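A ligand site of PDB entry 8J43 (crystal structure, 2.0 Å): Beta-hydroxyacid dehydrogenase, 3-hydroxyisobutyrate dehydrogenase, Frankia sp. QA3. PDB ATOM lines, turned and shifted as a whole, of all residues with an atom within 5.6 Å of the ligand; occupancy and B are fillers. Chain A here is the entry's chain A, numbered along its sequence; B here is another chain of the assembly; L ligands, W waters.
Gly 12 touches the ligand.
Val 74 touches the ligand.
CG1 of Val 78 touches C9 of the ligand (3.7 Å).
CG2 of Thr 95 touches O12 of the ligand (3.96 Å).
Ile 121 touches the ligand (O to C20, 3.4 Å).
Thr 123 touches the ligand.
Thr 124 touches the ligand (CA to O14, 3.5 Å).
CD of Pro 125 touches O14 of the ligand (3.3 Å).
Ala 234 of chain B touches the ligand (CB to O14, 3.4 Å).
CG2 of Val 238 of chain B touches O7 of the ligand (3.4 Å).
Of the 31 residues printed, 23 come within 4 Å of the ligand.
O of Val 238 of chain B is in hydrogen-bond range of OG of Ser 242 of chain B (3.4 Å).
The side-chain amide oxygen (OD1) of Asn 35 is in hydrogen-bond range of the backbone NH (N) of Leu 13.
The backbone NH (N) of Gly 12 sits at hydrogen-bond distance from the backbone carbonyl oxygen (O) of Trp 34, 2.9 Å away.
The side-chain hydroxyl (OG1) of Thr 95 sits at hydrogen-bond distance from the backbone NH (N) of Val 69, 3.2 Å away.
The backbone carbonyl oxygen (O) of Ser 37 sits at hydrogen-bond distance from the side-chain amide nitrogen (ND2) of Asn 35.
The side-chain carboxylate of Asp 71 lies within hydrogen-bond range of the backbone NH of Val 74 (3.1 Å).
OG1 of Thr 235 of chain B sits at hydrogen-bond distance from N of Val 238 of chain B, at 3.2 Å.
Water W8 lies within hydrogen-bond range of O9 of the ligand (2.7 Å), O of Cys 68 (2.9 Å), N of Gly 14 (2.9 Å) and N of Gly 17 (3.0 Å).
Water W3 lies within hydrogen-bond range of an oxygen (O1) of the ligand (2.8 Å) and the side-chain amino group of Lys 40 (3.0 Å).
Water W4 lies within hydrogen-bond range of OG of Ser 242 of chain B (2.8 Å) and O13 of the ligand (2.8 Å).
Water W7 lies within hydrogen-bond range of the backbone carbonyl oxygen (O) of Val 238 of chain B, an oxygen (O13) of the ligand and the backbone NH (N) of Ser 242 of chain B.
Water W1 lies within hydrogen-bond range of N of Arg 36 (2.9 Å), OD1 of Asn 35 (3.0 Å) and N5 of the ligand (3.1 Å).
Water W2 lies within hydrogen-bond range of O of Leu 94 (2.9 Å) and N of Ile 121 (3.0 Å).
NH2 of Arg 36 lies within salt-bridge range of O15 of the ligand.
O12 of the ligand lies within hydrogen-bond range of O of Leu 70, at 2.8 Å.
An oxygen (O17) of the ligand lies within hydrogen-bond range of the side-chain hydroxyl of Ser 37 (2.6 Å).
O of Val 69 sits close to O12 of the ligand.
An oxygen (O5) of the ligand is in hydrogen-bond range of the side-chain amide oxygen (OD1) of Asn 35 (2.7 Å).
An oxygen (O12) of the ligand is in hydrogen-bond range of the backbone NH (N) of Ser 96 (3.0 Å).
N of Leu 15 is in hydrogen-bond range of O1 of the ligand, 2.8 Å away.
N of Gly 14 sits at hydrogen-bond distance from O5 of the ligand.
An oxygen (O4) of the ligand is in hydrogen-bond range of the backbone NH (N) of Leu 70 (3.0 Å).
The backbone NH (N) of Met 16 lies within hydrogen-bond range of an oxygen (O9) of the ligand (2.9 Å).
An oxygen (O5) of the ligand is in hydrogen-bond range of the backbone NH (N) of Leu 13 (3.4 Å).
NZ of Lys 40 lies within salt-bridge range of O16 of the ligand (2.6 Å).
The side-chain hydroxyl of Ser 96 sits at hydrogen-bond distance from an oxygen (O13) of the ligand, 2.6 Å away.
The backbone NH (N) of Ser 37 sits at hydrogen-bond distance from an oxygen (O17) of the ligand, 3.0 Å away.
The side-chain sulfur (SG) of Cys 68 sits at hydrogen-bond distance from an oxygen (O11) of the ligand (3.4 Å).
The backbone carbonyl oxygen (O) of Asp 233 of chain B is in hydrogen-bond range of a nitrogen (N7) of the ligand (2.9 Å).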
ATOM      1  N   GLY A  12     -24.304  14.532  12.780  1.00  0.00           N
ATOM      2  CA  GLY A  12     -24.439  13.138  12.366  1.00  0.00           C
ATOM      3  C   GLY A  12     -25.629  12.530  13.095  1.00  0.00           C
ATOM      4  O   GLY A  12     -25.629  12.489  14.323  1.00  0.00           O
ATOM      5  N   LEU A  13     -26.639  12.127  12.338  1.00  0.00           N
ATOM      6  CA  LEU A  13     -27.859  11.553  12.886  1.00  0.00           C
ATOM      7  C   LEU A  13     -28.116  10.161  12.321  1.00  0.00           C
ATOM      8  O   LEU A  13     -29.245   9.821  11.942  1.00  0.00           O
ATOM      9  CB  LEU A  13     -29.037  12.478  12.634  1.00  0.00           C
ATOM     10  CG  LEU A  13     -28.910  13.869  13.269  1.00  0.00           C
ATOM     11  CD1 LEU A  13     -30.053  14.771  12.831  1.00  0.00           C
ATOM     12  CD2 LEU A  13     -28.840  13.781  14.784  1.00  0.00           C
ATOM     13  N   GLY A  14     -27.059   9.352  12.281  1.00  0.00           N
ATOM     14  CA  GLY A  14     -27.180   7.917  12.008  1.00  0.00           C
ATOM     15  C   GLY A  14     -27.830   7.203  13.190  1.00  0.00           C
ATOM     16  O   GLY A  14     -28.384   7.835  14.084  1.00  0.00           O
ATOM     17  N   LEU A  15     -27.743   5.880  13.175  1.00  0.00           N
ATOM     18  CA  LEU A  15     -28.265   5.071  14.268  1.00  0.00           C
ATOM     19  C   LEU A  15     -27.725   5.543  15.606  1.00  0.00           C
ATOM     20  O   LEU A  15     -28.489   5.670  16.559  1.00  0.00           O
ATOM     21  CB  LEU A  15     -27.971   3.577  14.065  1.00  0.00           C
ATOM     22  CG  LEU A  15     -28.497   2.990  12.747  1.00  0.00           C
ATOM     23  CD1 LEU A  15     -28.039   1.568  12.542  1.00  0.00           C
ATOM     24  CD2 LEU A  15     -30.025   3.147  12.695  1.00  0.00           C
ATOM     25  N   MET A  16     -26.432   5.844  15.676  1.00  0.00           N
ATOM     26  CA  MET A  16     -25.843   6.275  16.948  1.00  0.00           C
ATOM     27  C   MET A  16     -26.044   7.766  17.228  1.00  0.00           C
ATOM     28  O   MET A  16     -26.400   8.148  18.329  1.00  0.00           O
ATOM     29  CB  MET A  16     -24.353   5.929  17.015  1.00  0.00           C
ATOM     30  CG  MET A  16     -23.679   6.331  18.314  1.00  0.00           C
ATOM     31  SD  MET A  16     -24.478   5.732  19.827  1.00  0.00           S
ATOM     32  CE  MET A  16     -23.981   4.016  19.787  1.00  0.00           C
ATOM     33  N   GLY A  17     -25.775   8.599  16.247  1.00  0.00           N
ATOM     34  CA  GLY A  17     -25.961  10.049  16.375  1.00  0.00           C
ATOM     35  C   GLY A  17     -27.360  10.450  16.843  1.00  0.00           C
ATOM     36  O   GLY A  17     -27.511  11.330  17.709  1.00  0.00           O
ATOM     37  N   TRP A  34     -27.502  18.416  12.861  1.00  0.00           N
ATOM     38  CA  TRP A  34     -27.318  18.408  11.443  1.00  0.00           C
ATOM     39  C   TRP A  34     -26.971  17.015  10.976  1.00  0.00           C
ATOM     40  O   TRP A  34     -26.251  16.286  11.643  1.00  0.00           O
ATOM     41  CB  TRP A  34     -26.193  19.350  11.026  1.00  0.00           C
ATOM     42  CG  TRP A  34     -26.038  19.378   9.545  1.00  0.00           C
ATOM     43  CD1 TRP A  34     -26.737  20.150   8.669  1.00  0.00           C
ATOM     44  CD2 TRP A  34     -25.178  18.557   8.751  1.00  0.00           C
ATOM     45  NE1 TRP A  34     -26.332  19.881   7.378  1.00  0.00           N
ATOM     46  CE2 TRP A  34     -25.385  18.912   7.403  1.00  0.00           C
ATOM     47  CE3 TRP A  34     -24.222  17.569   9.059  1.00  0.00           C
ATOM     48  CZ2 TRP A  34     -24.676  18.316   6.353  1.00  0.00           C
ATOM     49  CZ3 TRP A  34     -23.515  16.985   8.002  1.00  0.00           C
ATOM     50  CH2 TRP A  34     -23.748  17.359   6.669  1.00  0.00           C
ATOM     51  N   ASN A  35     -27.473  16.682   9.796  1.00  0.00           N
ATOM     52  CA  ASN A  35     -27.110  15.456   9.113  1.00  0.00           C
ATOM     53  C   ASN A  35     -27.199  15.715   7.612  1.00  0.00           C
ATOM     54  O   ASN A  35     -28.034  16.499   7.174  1.00  0.00           O
ATOM     55  CB  ASN A  35     -28.070  14.349   9.544  1.00  0.00           C
ATOM     56  CG  ASN A  35     -27.627  12.986   9.060  1.00  0.00           C
ATOM     57  OD1 ASN A  35     -26.571  12.495   9.439  1.00  0.00           O
ATOM     58  ND2 ASN A  35     -28.455  12.357   8.222  1.00  0.00           N
ATOM     59  N   ARG A  36     -26.315  15.095   6.815  1.00  0.00           N
ATOM     60  CA  ARG A  36     -26.382  15.188   5.358  1.00  0.00           C
ATOM     61  C   ARG A  36     -27.788  14.893   4.835  1.00  0.00           C
ATOM     62  O   ARG A  36     -28.328  15.671   4.064  1.00  0.00           O
ATOM     63  CB  ARG A  36     -25.367  14.226   4.729  1.00  0.00           C
ATOM     64  CG  ARG A  36     -25.451  14.093   3.208  1.00  0.00           C
ATOM     65  CD  ARG A  36     -24.393  13.138   2.677  1.00  0.00           C
ATOM     66  NE  ARG A  36     -24.578  11.774   3.215  1.00  0.00           N
ATOM     67  CZ  ARG A  36     -23.952  10.694   2.777  1.00  0.00           C
ATOM     68  NH1 ARG A  36     -23.081  10.768   1.776  1.00  0.00           N
ATOM     69  NH2 ARG A  36     -24.190   9.525   3.338  1.00  0.00           N
ATOM     70  N   SER A  37     -28.388  13.790   5.275  1.00  0.00           N
ATOM     71  CA  SER A  37     -29.789  13.493   4.955  1.00  0.00           C
ATOM     72  C   SER A  37     -30.708  14.049   6.021  1.00  0.00           C
ATOM     73  O   SER A  37     -30.868  13.455   7.081  1.00  0.00           O
ATOM     74  CB  SER A  37     -30.005  11.984   4.834  1.00  0.00           C
ATOM     75  OG  SER A  37     -29.013  11.402   4.047  1.00  0.00           O
ATOM     76  N   LYS A  40     -33.605  12.190   8.374  1.00  0.00           N
ATOM     77  CA  LYS A  40     -33.289  11.474   9.617  1.00  0.00           C
ATOM     78  C   LYS A  40     -33.471  12.313  10.863  1.00  0.00           C
ATOM     79  O   LYS A  40     -33.548  11.754  11.968  1.00  0.00           O
ATOM     80  CB  LYS A  40     -31.860  10.900   9.565  1.00  0.00           C
ATOM     81  CG  LYS A  40     -31.731   9.839   8.483  1.00  0.00           C
ATOM     82  CD  LYS A  40     -30.413   9.114   8.562  1.00  0.00           C
ATOM     83  CE  LYS A  40     -30.200   8.334   7.281  1.00  0.00           C
ATOM     84  NZ  LYS A  40     -28.959   7.541   7.377  1.00  0.00           N
ATOM     85  N   CYS A  68     -20.554  12.456  15.373  1.00  0.00           N
ATOM     86  CA  CYS A  68     -20.663  11.003  15.301  1.00  0.00           C
ATOM     87  C   CYS A  68     -21.083  10.647  13.886  1.00  0.00           C
ATOM     88  O   CYS A  68     -22.283  10.498  13.594  1.00  0.00           O
ATOM     89  CB  CYS A  68     -21.643  10.476  16.338  1.00  0.00           C
ATOM     90  SG  CYS A  68     -21.681   8.671  16.434  1.00  0.00           S
ATOM     91  N   VAL A  69     -20.098  10.577  13.009  1.00  0.00           N
ATOM     92  CA  VAL A  69     -20.305  10.261  11.591  1.00  0.00           C
ATOM     93  C   VAL A  69     -19.574   8.968  11.255  1.00  0.00           C
ATOM     94  O   VAL A  69     -18.962   8.362  12.140  1.00  0.00           O
ATOM     95  CB  VAL A  69     -19.848  11.436  10.680  1.00  0.00           C
ATOM     96  CG1 VAL A  69     -20.739  12.651  10.894  1.00  0.00           C
ATOM     97  CG2 VAL A  69     -18.369  11.792  10.917  1.00  0.00           C
ATOM     98  N   LEU A  70     -19.632   8.527  10.004  1.00  0.00           N
ATOM     99  CA  LEU A  70     -19.041   7.238   9.638  1.00  0.00           C
ATOM    100  C   LEU A  70     -17.571   7.106  10.065  1.00  0.00           C
ATOM    101  O   LEU A  70     -17.208   6.161  10.779  1.00  0.00           O
ATOM    102  CB  LEU A  70     -19.197   6.940   8.142  1.00  0.00           C
ATOM    103  CG  LEU A  70     -18.611   5.592   7.658  1.00  0.00           C
ATOM    104  CD1 LEU A  70     -19.183   4.435   8.497  1.00  0.00           C
ATOM    105  CD2 LEU A  70     -18.855   5.340   6.172  1.00  0.00           C
ATOM    106  N   ASP A  71     -16.739   8.042   9.600  1.00  0.00           N
ATOM    107  CA  ASP A  71     -15.306   8.011   9.873  1.00  0.00           C
ATOM    108  C   ASP A  71     -14.732   9.423   9.844  1.00  0.00           C
ATOM    109  O   ASP A  71     -15.454  10.380   9.561  1.00  0.00           O
ATOM    110  CB  ASP A  71     -14.567   7.110   8.859  1.00  0.00           C
ATOM    111  CG  ASP A  71     -14.697   7.597   7.431  1.00  0.00           C
ATOM    112  OD1 ASP A  71     -14.596   8.823   7.172  1.00  0.00           O
ATOM    113  OD2 ASP A  71     -14.939   6.745   6.552  1.00  0.00           O
ATOM    114  N   VAL A  74     -14.964  11.850   6.731  1.00  0.00           N
ATOM    115  CA  VAL A  74     -16.270  12.525   6.690  1.00  0.00           C
ATOM    116  C   VAL A  74     -16.309  13.694   7.673  1.00  0.00           C
ATOM    117  O   VAL A  74     -16.827  14.752   7.335  1.00  0.00           O
ATOM    118  CB  VAL A  74     -17.428  11.556   6.998  1.00  0.00           C
ATOM    119  CG1 VAL A  74     -18.744  12.319   7.140  1.00  0.00           C
ATOM    120  CG2 VAL A  74     -17.514  10.467   5.913  1.00  0.00           C
ATOM    121  N   SER A  77     -14.417  16.485   6.143  1.00  0.00           N
ATOM    122  CA  SER A  77     -15.203  16.910   5.009  1.00  0.00           C
ATOM    123  C   SER A  77     -16.357  17.844   5.446  1.00  0.00           C
ATOM    124  O   SER A  77     -16.513  18.926   4.897  1.00  0.00           O
ATOM    125  CB  SER A  77     -15.703  15.679   4.267  1.00  0.00           C
ATOM    126  OG  SER A  77     -16.414  16.056   3.141  1.00  0.00           O
ATOM    127  N   VAL A  78     -17.125  17.452   6.463  1.00  0.00           N
ATOM    128  CA  VAL A  78     -18.279  18.275   6.888  1.00  0.00           C
ATOM    129  C   VAL A  78     -17.887  19.452   7.780  1.00  0.00           C
ATOM    130  O   VAL A  78     -18.618  20.426   7.874  1.00  0.00           O
ATOM    131  CB  VAL A  78     -19.396  17.459   7.573  1.00  0.00           C
ATOM    132  CG1 VAL A  78     -19.781  16.247   6.721  1.00  0.00           C
ATOM    133  CG2 VAL A  78     -18.986  17.013   8.980  1.00  0.00           C
ATOM    134  N   LEU A  94     -17.015  11.350  18.744  1.00  0.00           N
ATOM    135  CA  LEU A  94     -17.403   9.976  19.100  1.00  0.00           C
ATOM    136  C   LEU A  94     -17.463   9.105  17.865  1.00  0.00           C
ATOM    137  O   LEU A  94     -17.975   7.976  17.885  1.00  0.00           O
ATOM    138  CB  LEU A  94     -18.754   9.946  19.842  1.00  0.00           C
ATOM    139  CG  LEU A  94     -18.851  10.759  21.137  1.00  0.00           C
ATOM    140  CD1 LEU A  94     -20.256  10.696  21.715  1.00  0.00           C
ATOM    141  CD2 LEU A  94     -17.812  10.283  22.136  1.00  0.00           C
ATOM    142  N   THR A  95     -16.896   9.620  16.775  1.00  0.00           N
ATOM    143  CA  THR A  95     -16.694   8.845  15.571  1.00  0.00           C
ATOM    144  C   THR A  95     -15.652   7.734  15.828  1.00  0.00           C
ATOM    145  O   THR A  95     -14.734   7.926  16.621  1.00  0.00           O
ATOM    146  CB  THR A  95     -16.223   9.767  14.432  1.00  0.00           C
ATOM    147  OG1 THR A  95     -17.183  10.834  14.254  1.00  0.00           O
ATOM    148  CG2 THR A  95     -16.038   8.992  13.137  1.00  0.00           C
ATOM    149  N   SER A  96     -15.844   6.567  15.199  1.00  0.00           N
ATOM    150  CA  SER A  96     -14.873   5.493  15.278  1.00  0.00           C
ATOM    151  C   SER A  96     -13.666   5.867  14.409  1.00  0.00           C
ATOM    152  O   SER A  96     -13.815   6.470  13.336  1.00  0.00           O
ATOM    153  CB  SER A  96     -15.465   4.152  14.811  1.00  0.00           C
ATOM    154  OG  SER A  96     -16.561   3.733  15.620  1.00  0.00           O
ATOM    155  N   ILE A 121     -17.730   4.982  22.042  1.00  0.00           N
ATOM    156  CA  ILE A 121     -19.013   4.564  22.637  1.00  0.00           C
ATOM    157  C   ILE A 121     -19.027   3.027  22.784  1.00  0.00           C
ATOM    158  O   ILE A 121     -19.059   2.299  21.783  1.00  0.00           O
ATOM    159  CB  ILE A 121     -20.184   5.008  21.744  1.00  0.00           C
ATOM    160  CG1 ILE A 121     -20.154   6.522  21.497  1.00  0.00           C
ATOM    161  CG2 ILE A 121     -21.502   4.641  22.372  1.00  0.00           C
ATOM    162  CD1 ILE A 121     -21.016   6.984  20.348  1.00  0.00           C
ATOM    163  N   MET A 122     -19.001   2.524  24.019  1.00  0.00           N
ATOM    164  CA  MET A 122     -18.996   1.066  24.223  1.00  0.00           C
ATOM    165  C   MET A 122     -20.407   0.567  24.548  1.00  0.00           C
ATOM    166  O   MET A 122     -20.697   0.051  25.645  1.00  0.00           O
ATOM    167  CB  MET A 122     -17.951   0.641  25.275  1.00  0.00           C
ATOM    168  CG  MET A 122     -16.587   1.287  25.102  1.00  0.00           C
ATOM    169  SD  MET A 122     -15.938   1.227  23.399  1.00  0.00           S
ATOM    170  CE  MET A 122     -15.882  -0.553  23.127  1.00  0.00           C
ATOM    171  N   THR A 123     -21.295   0.742  23.567  1.00  0.00           N
ATOM    172  CA  THR A 123     -22.698   0.301  23.636  1.00  0.00           C
ATOM    173  C   THR A 123     -23.326   0.496  22.259  1.00  0.00           C
ATOM    174  O   THR A 123     -22.823   1.291  21.434  1.00  0.00           O
ATOM    175  CB  THR A 123     -23.528   1.075  24.697  1.00  0.00           C
ATOM    176  OG1 THR A 123     -24.882   0.597  24.722  1.00  0.00           O
ATOM    177  CG2 THR A 123     -23.532   2.610  24.438  1.00  0.00           C
ATOM    178  N   THR A 124     -24.418  -0.225  21.998  1.00  0.00           N
ATOM    179  CA  THR A 124     -25.249   0.070  20.840  1.00  0.00           C
ATOM    180  C   THR A 124     -26.204   1.205  21.235  1.00  0.00           C
ATOM    181  O   THR A 124     -26.226   1.614  22.381  1.00  0.00           O
ATOM    182  CB  THR A 124     -25.996  -1.179  20.382  1.00  0.00           C
ATOM    183  OG1 THR A 124     -26.639  -1.787  21.487  1.00  0.00           O
ATOM    184  CG2 THR A 124     -25.044  -2.193  19.781  1.00  0.00           C
ATOM    185  N   PRO A 125     -27.006   1.723  20.278  1.00  0.00           N
ATOM    186  CA  PRO A 125     -27.815   2.909  20.600  1.00  0.00           C
ATOM    187  C   PRO A 125     -28.780   2.824  21.787  1.00  0.00           C
ATOM    188  O   PRO A 125     -28.921   3.810  22.495  1.00  0.00           O
ATOM    189  CB  PRO A 125     -28.556   3.185  19.279  1.00  0.00           C
ATOM    190  CG  PRO A 125     -27.546   2.767  18.254  1.00  0.00           C
ATOM    191  CD  PRO A 125     -26.922   1.511  18.818  1.00  0.00           C
ATOM    192  N   ASP B 233     -29.739  -1.367  15.383  1.00  0.00           N
ATOM    193  CA  ASP B 233     -28.738  -0.955  16.355  1.00  0.00           C
ATOM    194  C   ASP B 233     -27.395  -0.619  15.705  1.00  0.00           C
ATOM    195  O   ASP B 233     -26.839   0.473  15.920  1.00  0.00           O
ATOM    196  CB  ASP B 233     -28.601  -2.011  17.497  1.00  0.00           C
ATOM    197  CG  ASP B 233     -28.270  -3.435  16.988  1.00  0.00           C
ATOM    198  OD1 ASP B 233     -28.449  -3.742  15.790  1.00  0.00           O
ATOM    199  OD2 ASP B 233     -27.825  -4.275  17.825  1.00  0.00           O
ATOM    200  N   ALA B 234     -26.886  -1.547  14.903  1.00  0.00           N
ATOM    201  CA  ALA B 234     -25.645  -1.347  14.169  1.00  0.00           C
ATOM    202  C   ALA B 234     -25.604  -2.302  12.991  1.00  0.00           C
ATOM    203  O   ALA B 234     -26.054  -3.459  13.111  1.00  0.00           O
ATOM    204  CB  ALA B 234     -24.479  -1.604  15.087  1.00  0.00           C
ATOM    205  N   THR B 235     -25.049  -1.842  11.873  1.00  0.00           N
ATOM    206  CA  THR B 235     -25.094  -2.594  10.618  1.00  0.00           C
ATOM    207  C   THR B 235     -23.768  -3.256  10.273  1.00  0.00           C
ATOM    208  O   THR B 235     -22.686  -2.809  10.692  1.00  0.00           O
ATOM    209  CB  THR B 235     -25.477  -1.694   9.431  1.00  0.00           C
ATOM    210  OG1 THR B 235     -24.459  -0.728   9.226  1.00  0.00           O
ATOM    211  CG2 THR B 235     -26.810  -0.965   9.685  1.00  0.00           C
ATOM    212  N   VAL B 238     -21.281  -0.878   8.669  1.00  0.00           N
ATOM    213  CA  VAL B 238     -20.612   0.023   9.591  1.00  0.00           C
ATOM    214  C   VAL B 238     -19.484  -0.703  10.313  1.00  0.00           C
ATOM    215  O   VAL B 238     -18.426  -0.129  10.561  1.00  0.00           O
ATOM    216  CB  VAL B 238     -21.607   0.680  10.581  1.00  0.00           C
ATOM    217  CG1 VAL B 238     -20.913   1.299  11.798  1.00  0.00           C
ATOM    218  CG2 VAL B 238     -22.438   1.749   9.849  1.00  0.00           C
ATOM    219  N   SER B 242     -15.325  -0.181  10.681  1.00  0.00           N
ATOM    220  CA  SER B 242     -14.598  -0.058  11.945  1.00  0.00           C
ATOM    221  C   SER B 242     -13.578  -1.162  12.142  1.00  0.00           C
ATOM    222  O   SER B 242     -12.542  -0.893  12.732  1.00  0.00           O
ATOM    223  CB  SER B 242     -15.497   0.133  13.186  1.00  0.00           C
ATOM    224  OG  SER B 242     -16.459  -0.871  13.280  1.00  0.00           O
HETATM  225  P1  LIG L   1     -24.843   5.106  10.369  1.00  0.00           P
HETATM  226  O1  LIG L   1     -26.240   4.990  10.950  1.00  0.00           O
HETATM  227  O2  LIG L   1     -24.471   4.537   9.014  1.00  0.00           O
HETATM  228  O3  LIG L   1     -24.427   6.643  10.321  1.00  0.00           O
HETATM  229  C1  LIG L   1     -23.432   7.142   9.433  1.00  0.00           C
HETATM  230  C2  LIG L   1     -23.408   8.651   9.596  1.00  0.00           C
HETATM  231  O4  LIG L   1     -22.353   9.237   8.851  1.00  0.00           O
HETATM  232  C3  LIG L   1     -24.691   9.274   9.071  1.00  0.00           C
HETATM  233  O5  LIG L   1     -24.976  10.414   9.861  1.00  0.00           O
HETATM  234  C4  LIG L   1     -24.331   9.645   7.656  1.00  0.00           C
HETATM  235  O6  LIG L   1     -25.220  10.603   7.073  1.00  0.00           O
HETATM  236  C5  LIG L   1     -22.913  10.132   7.856  1.00  0.00           C
HETATM  237  N1  LIG L   1     -22.111  10.112   6.605  1.00  0.00           N
HETATM  238  C6  LIG L   1     -21.563   9.027   6.005  1.00  0.00           C
HETATM  239  N2  LIG L   1     -20.892   9.387   4.888  1.00  0.00           N
HETATM  240  C7  LIG L   1     -21.006  10.724   4.779  1.00  0.00           C
HETATM  241  C8  LIG L   1     -20.520  11.757   3.846  1.00  0.00           C
HETATM  242  N3  LIG L   1     -19.783  11.394   2.792  1.00  0.00           N
HETATM  243  N4  LIG L   1     -20.850  13.049   4.070  1.00  0.00           N
HETATM  244  C9  LIG L   1     -21.605  13.387   5.126  1.00  0.00           C
HETATM  245  N5  LIG L   1     -22.063  12.487   6.015  1.00  0.00           N
HETATM  246  C10 LIG L   1     -21.805  11.184   5.904  1.00  0.00           C
HETATM  247  O7  LIG L   1     -23.789   4.483  11.437  1.00  0.00           O
HETATM  248  P2  LIG L   1     -23.761   4.829  13.021  1.00  0.00           P
HETATM  249  O8  LIG L   1     -23.945   3.464  13.653  1.00  0.00           O
HETATM  250  O9  LIG L   1     -24.622   6.010  13.415  1.00  0.00           O
HETATM  251  O10 LIG L   1     -22.242   5.150  13.384  1.00  0.00           O
HETATM  252  C11 LIG L   1     -21.513   6.353  13.172  1.00  0.00           C
HETATM  253  C12 LIG L   1     -20.214   6.147  13.940  1.00  0.00           C
HETATM  254  O11 LIG L   1     -20.533   5.676  15.252  1.00  0.00           O
HETATM  255  C13 LIG L   1     -19.328   5.079  13.332  1.00  0.00           C
HETATM  256  O12 LIG L   1     -17.991   5.559  13.429  1.00  0.00           O
HETATM  257  C14 LIG L   1     -19.585   3.825  14.180  1.00  0.00           C
HETATM  258  O13 LIG L   1     -18.508   2.890  14.202  1.00  0.00           O
HETATM  259  C15 LIG L   1     -19.804   4.473  15.535  1.00  0.00           C
HETATM  260  N6  LIG L   1     -20.461   3.621  16.537  1.00  0.00           N
HETATM  261  C16 LIG L   1     -21.643   3.021  16.291  1.00  0.00           C
HETATM  262  C17 LIG L   1     -22.264   2.210  17.234  1.00  0.00           C
HETATM  263  C18 LIG L   1     -23.585   1.527  16.947  1.00  0.00           C
HETATM  264  O14 LIG L   1     -23.932   0.590  17.643  1.00  0.00           O
HETATM  265  N7  LIG L   1     -24.385   1.947  15.985  1.00  0.00           N
HETATM  266  C19 LIG L   1     -21.642   2.023  18.452  1.00  0.00           C
HETATM  267  C20 LIG L   1     -20.434   2.656  18.707  1.00  0.00           C
HETATM  268  C21 LIG L   1     -19.864   3.460  17.733  1.00  0.00           C
HETATM  269  P3  LIG L   1     -26.495  10.047   6.202  1.00  0.00           P
HETATM  270  O15 LIG L   1     -25.962   8.856   5.440  1.00  0.00           O
HETATM  271  O16 LIG L   1     -27.516   9.682   7.258  1.00  0.00           O
HETATM  272  O17 LIG L   1     -26.821  11.280   5.383  1.00  0.00           O
HETATM  273  O   HOH W   1     -24.157  13.588   7.966  1.00  0.00           O
HETATM  274  O   HOH W   2     -17.478   5.428  19.100  1.00  0.00           O
HETATM  275  O   HOH W   3     -28.612   5.731   9.766  1.00  0.00           O
HETATM  276  O   HOH W   4     -18.531   0.129  14.825  1.00  0.00           O
HETATM  277  O   HOH W   5     -22.393   5.548   6.636  1.00  0.00           O
HETATM  278  O   HOH W   6     -24.791   6.519   5.331  1.00  0.00           O
HETATM  279  O   HOH W   7     -17.520   2.429  11.445  1.00  0.00           O
HETATM  280  O   HOH W   8     -24.536   8.751  13.558  1.00  0.00           O
